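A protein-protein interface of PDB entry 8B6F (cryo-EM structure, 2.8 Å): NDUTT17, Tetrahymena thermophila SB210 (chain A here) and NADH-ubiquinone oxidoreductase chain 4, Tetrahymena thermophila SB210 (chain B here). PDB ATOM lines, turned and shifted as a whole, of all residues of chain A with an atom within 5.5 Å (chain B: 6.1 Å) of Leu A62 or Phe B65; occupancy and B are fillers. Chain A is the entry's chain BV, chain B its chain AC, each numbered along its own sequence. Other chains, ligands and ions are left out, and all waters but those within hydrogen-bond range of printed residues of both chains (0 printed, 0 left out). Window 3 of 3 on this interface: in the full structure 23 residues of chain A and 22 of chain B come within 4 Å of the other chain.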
ATOM      1  N   ALA A  57      22.589 -14.205 -15.701  1.00  0.00           N
ATOM      2  CA  ALA A  57      21.155 -14.286 -15.455  1.00  0.00           C
ATOM      3  C   ALA A  57      20.875 -14.625 -13.996  1.00  0.00           C
ATOM      4  O   ALA A  57      20.024 -14.001 -13.353  1.00  0.00           O
ATOM      5  CB  ALA A  57      20.523 -15.325 -16.381  1.00  0.00           C
ATOM      6  N   VAL A  58      21.585 -15.619 -13.457  1.00  0.00           N
ATOM      7  CA  VAL A  58      21.333 -16.057 -12.085  1.00  0.00           C
ATOM      8  C   VAL A  58      21.636 -14.933 -11.104  1.00  0.00           C
ATOM      9  O   VAL A  58      20.848 -14.645 -10.196  1.00  0.00           O
ATOM     10  CB  VAL A  58      22.154 -17.320 -11.767  1.00  0.00           C
ATOM     11  CG1 VAL A  58      22.172 -17.601 -10.266  1.00  0.00           C
ATOM     12  CG2 VAL A  58      21.597 -18.515 -12.518  1.00  0.00           C
ATOM     13  N   ALA A  59      22.788 -14.283 -11.270  1.00  0.00           N
ATOM     14  CA  ALA A  59      23.178 -13.234 -10.335  1.00  0.00           C
ATOM     15  C   ALA A  59      22.243 -12.037 -10.422  1.00  0.00           C
ATOM     16  O   ALA A  59      21.846 -11.477  -9.393  1.00  0.00           O
ATOM     17  CB  ALA A  59      24.621 -12.813 -10.596  1.00  0.00           C
ATOM     18  N   GLY A  60      21.883 -11.624 -11.638  1.00  0.00           N
ATOM     19  CA  GLY A  60      20.953 -10.518 -11.777  1.00  0.00           C
ATOM     20  C   GLY A  60      19.594 -10.827 -11.181  1.00  0.00           C
ATOM     21  O   GLY A  60      19.003  -9.991 -10.494  1.00  0.00           O
ATOM     22  N   LEU A  61      19.083 -12.034 -11.430  1.00  0.00           N
ATOM     23  CA  LEU A  61      17.793 -12.419 -10.869  1.00  0.00           C
ATOM     24  C   LEU A  61      17.843 -12.458  -9.348  1.00  0.00           C
ATOM     25  O   LEU A  61      16.924 -11.975  -8.676  1.00  0.00           O
ATOM     26  CB  LEU A  61      17.366 -13.774 -11.430  1.00  0.00           C
ATOM     27  CG  LEU A  61      17.003 -13.783 -12.914  1.00  0.00           C
ATOM     28  CD1 LEU A  61      16.941 -15.203 -13.438  1.00  0.00           C
ATOM     29  CD2 LEU A  61      15.678 -13.073 -13.143  1.00  0.00           C
ATOM     30  N   LEU A  62      18.913 -13.020  -8.782  1.00  0.00           N
ATOM     31  CA  LEU A  62      19.032 -13.057  -7.330  1.00  0.00           C
ATOM     32  C   LEU A  62      19.070 -11.652  -6.749  1.00  0.00           C
ATOM     33  O   LEU A  62      18.404 -11.368  -5.747  1.00  0.00           O
ATOM     34  CB  LEU A  62      20.283 -13.838  -6.923  1.00  0.00           C
ATOM     35  CG  LEU A  62      20.234 -15.361  -7.078  1.00  0.00           C
ATOM     36  CD1 LEU A  62      21.567 -15.967  -6.689  1.00  0.00           C
ATOM     37  CD2 LEU A  62      19.116 -15.971  -6.245  1.00  0.00           C
ATOM     38  N   SER A  63      19.850 -10.760  -7.357  1.00  0.00           N
ATOM     39  CA  SER A  63      19.936  -9.393  -6.855  1.00  0.00           C
ATOM     40  C   SER A  63      18.583  -8.700  -6.934  1.00  0.00           C
ATOM     41  O   SER A  63      18.149  -8.049  -5.976  1.00  0.00           O
ATOM     42  CB  SER A  63      20.992  -8.624  -7.644  1.00  0.00           C
ATOM     43  OG  SER A  63      22.250  -9.266  -7.525  1.00  0.00           O
ATOM     44  N   VAL A  64      17.904  -8.819  -8.075  1.00  0.00           N
ATOM     45  CA  VAL A  64      16.609  -8.164  -8.237  1.00  0.00           C
ATOM     46  C   VAL A  64      15.622  -8.697  -7.209  1.00  0.00           C
ATOM     47  O   VAL A  64      14.924  -7.932  -6.533  1.00  0.00           O
ATOM     48  CB  VAL A  64      16.085  -8.355  -9.673  1.00  0.00           C
ATOM     49  CG1 VAL A  64      14.633  -7.902  -9.788  1.00  0.00           C
ATOM     50  CG2 VAL A  64      16.945  -7.587 -10.654  1.00  0.00           C
ATOM     51  N   GLY A  65      15.557 -10.023  -7.068  1.00  0.00           N
ATOM     52  CA  GLY A  65      14.616 -10.607  -6.130  1.00  0.00           C
ATOM     53  C   GLY A  65      14.899 -10.202  -4.699  1.00  0.00           C
ATOM     54  O   GLY A  65      13.990  -9.830  -3.952  1.00  0.00           O
ATOM     55  N   SER A  66      16.167 -10.271  -4.292  1.00  0.00           N
ATOM     56  CA  SER A  66      16.514  -9.910  -2.923  1.00  0.00           C
ATOM     57  C   SER A  66      16.159  -8.459  -2.634  1.00  0.00           C
ATOM     58  O   SER A  66      15.487  -8.157  -1.641  1.00  0.00           O
ATOM     59  CB  SER A  66      18.004 -10.153  -2.683  1.00  0.00           C
ATOM     60  OG  SER A  66      18.347 -11.501  -2.949  1.00  0.00           O
ATOM     61  N   LEU A  67      16.574  -7.546  -3.513  1.00  0.00           N
ATOM     62  CA  LEU A  67      16.321  -6.128  -3.278  1.00  0.00           C
ATOM     63  C   LEU A  67      14.831  -5.821  -3.289  1.00  0.00           C
ATOM     64  O   LEU A  67      14.345  -5.044  -2.461  1.00  0.00           O
ATOM     65  CB  LEU A  67      17.060  -5.288  -4.321  1.00  0.00           C
ATOM     66  CG  LEU A  67      18.589  -5.339  -4.238  1.00  0.00           C
ATOM     67  CD1 LEU A  67      19.222  -4.550  -5.370  1.00  0.00           C
ATOM     68  CD2 LEU A  67      19.085  -4.823  -2.896  1.00  0.00           C
ATOM     69  N   ALA A 103      11.847 -13.939  -9.513  1.00  0.00           N
ATOM     70  CA  ALA A 103      13.280 -13.770  -9.720  1.00  0.00           C
ATOM     71  C   ALA A 103      14.063 -14.895  -9.054  1.00  0.00           C
ATOM     72  O   ALA A 103      14.920 -15.527  -9.679  1.00  0.00           O
ATOM     73  CB  ALA A 103      13.725 -12.410  -9.186  1.00  0.00           C
ATOM     74  N   ASN A 104      13.782 -15.157  -7.776  1.00  0.00           N
ATOM     75  CA  ASN A 104      14.506 -16.204  -7.062  1.00  0.00           C
ATOM     76  C   ASN A 104      14.272 -17.564  -7.703  1.00  0.00           C
ATOM     77  O   ASN A 104      15.204 -18.361  -7.851  1.00  0.00           O
ATOM     78  CB  ASN A 104      14.086 -16.233  -5.594  1.00  0.00           C
ATOM     79  CG  ASN A 104      14.414 -14.946  -4.868  1.00  0.00           C
ATOM     80  OD1 ASN A 104      15.425 -14.304  -5.145  1.00  0.00           O
ATOM     81  ND2 ASN A 104      13.561 -14.565  -3.928  1.00  0.00           N
ATOM     82  N   ALA A 107      16.208 -17.938 -10.955  1.00  0.00           N
ATOM     83  CA  ALA A 107      17.618 -18.186 -10.672  1.00  0.00           C
ATOM     84  C   ALA A 107      17.845 -19.640 -10.275  1.00  0.00           C
ATOM     85  O   ALA A 107      18.775 -20.291 -10.764  1.00  0.00           O
ATOM     86  CB  ALA A 107      18.100 -17.244  -9.568  1.00  0.00           C
ATOM     87  N   ILE B  60      27.007  -9.618   0.869  1.00  0.00           N
ATOM     88  CA  ILE B  60      27.354 -10.871   1.531  1.00  0.00           C
ATOM     89  C   ILE B  60      26.269 -11.916   1.298  1.00  0.00           C
ATOM     90  O   ILE B  60      26.554 -13.077   0.986  1.00  0.00           O
ATOM     91  CB  ILE B  60      27.586 -10.628   3.034  1.00  0.00           C
ATOM     92  CG1 ILE B  60      28.841  -9.778   3.253  1.00  0.00           C
ATOM     93  CG2 ILE B  60      27.692 -11.950   3.793  1.00  0.00           C
ATOM     94  CD1 ILE B  60      29.019  -9.292   4.683  1.00  0.00           C
ATOM     95  N   LEU B  61      25.004 -11.520   1.463  1.00  0.00           N
ATOM     96  CA  LEU B  61      23.899 -12.462   1.300  1.00  0.00           C
ATOM     97  C   LEU B  61      23.775 -12.982  -0.131  1.00  0.00           C
ATOM     98  O   LEU B  61      23.636 -14.190  -0.351  1.00  0.00           O
ATOM     99  CB  LEU B  61      22.593 -11.795   1.734  1.00  0.00           C
ATOM    100  CG  LEU B  61      21.368 -12.704   1.869  1.00  0.00           C
ATOM    101  CD1 LEU B  61      21.574 -13.766   2.938  1.00  0.00           C
ATOM    102  CD2 LEU B  61      20.122 -11.884   2.159  1.00  0.00           C
ATOM    103  N   ILE B  62      23.826 -12.089  -1.120  1.00  0.00           N
ATOM    104  CA  ILE B  62      23.731 -12.527  -2.513  1.00  0.00           C
ATOM    105  C   ILE B  62      24.943 -13.350  -2.927  1.00  0.00           C
ATOM    106  O   ILE B  62      24.813 -14.349  -3.642  1.00  0.00           O
ATOM    107  CB  ILE B  62      23.529 -11.320  -3.448  1.00  0.00           C
ATOM    108  CG1 ILE B  62      22.292 -10.522  -3.029  1.00  0.00           C
ATOM    109  CG2 ILE B  62      23.400 -11.787  -4.896  1.00  0.00           C
ATOM    110  CD1 ILE B  62      22.109  -9.231  -3.797  1.00  0.00           C
ATOM    111  N   SER B  63      26.136 -12.954  -2.491  1.00  0.00           N
ATOM    112  CA  SER B  63      27.309 -13.788  -2.719  1.00  0.00           C
ATOM    113  C   SER B  63      27.199 -15.137  -2.026  1.00  0.00           C
ATOM    114  O   SER B  63      27.718 -16.136  -2.535  1.00  0.00           O
ATOM    115  CB  SER B  63      28.555 -13.045  -2.256  1.00  0.00           C
ATOM    116  OG  SER B  63      28.701 -11.860  -3.013  1.00  0.00           O
ATOM    117  N   PHE B  64      26.526 -15.194  -0.879  1.00  0.00           N
ATOM    118  CA  PHE B  64      26.311 -16.481  -0.231  1.00  0.00           C
ATOM    119  C   PHE B  64      25.393 -17.368  -1.059  1.00  0.00           C
ATOM    120  O   PHE B  64      25.644 -18.571  -1.196  1.00  0.00           O
ATOM    121  CB  PHE B  64      25.742 -16.271   1.170  1.00  0.00           C
ATOM    122  CG  PHE B  64      25.341 -17.542   1.856  1.00  0.00           C
ATOM    123  CD1 PHE B  64      26.286 -18.504   2.170  1.00  0.00           C
ATOM    124  CD2 PHE B  64      24.021 -17.766   2.204  1.00  0.00           C
ATOM    125  CE1 PHE B  64      25.920 -19.671   2.805  1.00  0.00           C
ATOM    126  CE2 PHE B  64      23.646 -18.932   2.840  1.00  0.00           C
ATOM    127  CZ  PHE B  64      24.597 -19.886   3.142  1.00  0.00           C
ATOM    128  N   PHE B  65      24.332 -16.796  -1.631  1.00  0.00           N
ATOM    129  CA  PHE B  65      23.465 -17.572  -2.510  1.00  0.00           C
ATOM    130  C   PHE B  65      24.233 -18.082  -3.723  1.00  0.00           C
ATOM    131  O   PHE B  65      24.127 -19.255  -4.093  1.00  0.00           O
ATOM    132  CB  PHE B  65      22.275 -16.721  -2.949  1.00  0.00           C
ATOM    133  CG  PHE B  65      21.406 -16.259  -1.814  1.00  0.00           C
ATOM    134  CD1 PHE B  65      21.353 -16.964  -0.622  1.00  0.00           C
ATOM    135  CD2 PHE B  65      20.629 -15.122  -1.948  1.00  0.00           C
ATOM    136  CE1 PHE B  65      20.550 -16.536   0.417  1.00  0.00           C
ATOM    137  CE2 PHE B  65      19.823 -14.691  -0.913  1.00  0.00           C
ATOM    138  CZ  PHE B  65      19.782 -15.399   0.270  1.00  0.00           C
ATOM    139  N   ILE B  66      25.002 -17.203  -4.367  1.00  0.00           N
ATOM    140  CA  ILE B  66      25.804 -17.616  -5.515  1.00  0.00           C
ATOM    141  C   ILE B  66      26.820 -18.667  -5.097  1.00  0.00           C
ATOM    142  O   ILE B  66      27.146 -19.573  -5.874  1.00  0.00           O
ATOM    143  CB  ILE B  66      26.477 -16.395  -6.169  1.00  0.00           C
ATOM    144  CG1 ILE B  66      25.413 -15.414  -6.669  1.00  0.00           C
ATOM    145  CG2 ILE B  66      27.373 -16.832  -7.322  1.00  0.00           C
ATOM    146  CD1 ILE B  66      25.966 -14.081  -7.122  1.00  0.00           C
ATOM    147  N   HIS B  67      27.337 -18.569  -3.872  1.00  0.00           N
ATOM    148  CA  HIS B  67      28.276 -19.572  -3.381  1.00  0.00           C
ATOM    149  C   HIS B  67      27.594 -20.919  -3.190  1.00  0.00           C
ATOM    150  O   HIS B  67      28.198 -21.966  -3.450  1.00  0.00           O
ATOM    151  CB  HIS B  67      28.913 -19.110  -2.071  1.00  0.00           C
ATOM    152  CG  HIS B  67      29.763 -20.157  -1.419  1.00  0.00           C
ATOM    153  ND1 HIS B  67      30.879 -20.690  -2.026  1.00  0.00           N
ATOM    154  CD2 HIS B  67      29.654 -20.776  -0.220  1.00  0.00           C
ATOM    155  CE1 HIS B  67      31.424 -21.590  -1.227  1.00  0.00           C
ATOM    156  NE2 HIS B  67      30.699 -21.661  -0.126  1.00  0.00           N
ATOM    157  N   ILE B  68      26.342 -20.922  -2.730  1.00  0.00           N
ATOM    158  CA  ILE B  68      25.596 -22.175  -2.660  1.00  0.00           C
ATOM    159  C   ILE B  68      25.530 -22.814  -4.040  1.00  0.00           C
ATOM    160  O   ILE B  68      25.815 -24.005  -4.208  1.00  0.00           O
ATOM    161  CB  ILE B  68      24.187 -21.928  -2.091  1.00  0.00           C
ATOM    162  CG1 ILE B  68      24.276 -21.472  -0.635  1.00  0.00           C
ATOM    163  CG2 ILE B  68      23.330 -23.188  -2.204  1.00  0.00           C
ATOM    164  CD1 ILE B  68      22.948 -21.055  -0.039  1.00  0.00           C
ATOM    165  N   ILE B  69      25.151 -22.031  -5.048  1.00  0.00           N
ATOM    166  CA  ILE B  69      25.026 -22.568  -6.398  1.00  0.00           C
ATOM    167  C   ILE B  69      26.372 -23.093  -6.883  1.00  0.00           C
ATOM    168  O   ILE B  69      26.466 -24.184  -7.454  1.00  0.00           O
ATOM    169  CB  ILE B  69      24.453 -21.497  -7.344  1.00  0.00           C
ATOM    170  CG1 ILE B  69      23.004 -21.193  -6.959  1.00  0.00           C
ATOM    171  CG2 ILE B  69      24.541 -21.952  -8.793  1.00  0.00           C
ATOM    172  CD1 ILE B  69      22.382 -20.049  -7.729  1.00  0.00           C
ATOM    173  N   SER B  70      27.434 -22.314  -6.665  1.00  0.00           N
ATOM    174  CA  SER B  70      28.755 -22.707  -7.148  1.00  0.00           C
ATOM    175  C   SER B  70      29.275 -23.933  -6.407  1.00  0.00           C
ATOM    176  O   SER B  70      29.955 -24.779  -6.998  1.00  0.00           O
ATOM    177  CB  SER B  70      29.731 -21.539  -7.010  1.00  0.00           C
ATOM    178  OG  SER B  70      29.950 -21.209  -5.651  1.00  0.00           O
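Printed residues of chain A that touch a printed residue of chain B: Val A58, Ala A59, Leu A62 and Ser A63. Hydrophobic or aromatic side chains of chain B that line the printed part of chain A: Ile B62, Phe B65, Ile B66 and Ile B69. Along chain B the printed residues that touch a printed residue of chain A span positions 62 to 69. Among the printed residues, no Asp or Glu carboxylate lies within 4 Å of a Lys or Arg side-chain nitrogen of the other chain.
Val A58 touches Ile B69 (CG1 to CD1, 3.5 Å). CD1 of Ile B66 touches CB of Ala A59, 3.9 Å away. Leu A62 touches Phe B65 (CD1 to CB, 3.9 Å). Leu A62 touches Ile B66 (CD1 to CG1, 3.9 Å). Ile B62 touches Ser A63.
Printed residues of chain B within 4 Å of Val A58: Ile B69. Leu A61 touches none of the printed residues of chain B. Of the printed residues of chain A, Ile B62 touches Ser A63 (3.7 Å). Phe B65 touches just one residue of chain A: Leu A62. Printed residues of chain A within 4 Å of Ile B66: Ala A59 (3.9 Å) and Leu A62 (3.9 Å). Printed residues of chain A within 4 Å of Ile B69: Val A58 (3.5 Å). The nearest residue of chain B that does not touch Leu A62 is Ile B62 (4.2 Å). The nearest residue of chain A that does not touch Phe B65 is Ser A66 (4.1 Å).
OG of Ser B70 is in hydrogen-bond range of O of Ile B66 (3.3 Å). The side-chain hydroxyl of Ser A63 is in hydrogen-bond range of the backbone carbonyl oxygen of Ala A59. OG of Ser A66 sits at hydrogen-bond distance from O of Leu A62, 2.8 Å away.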
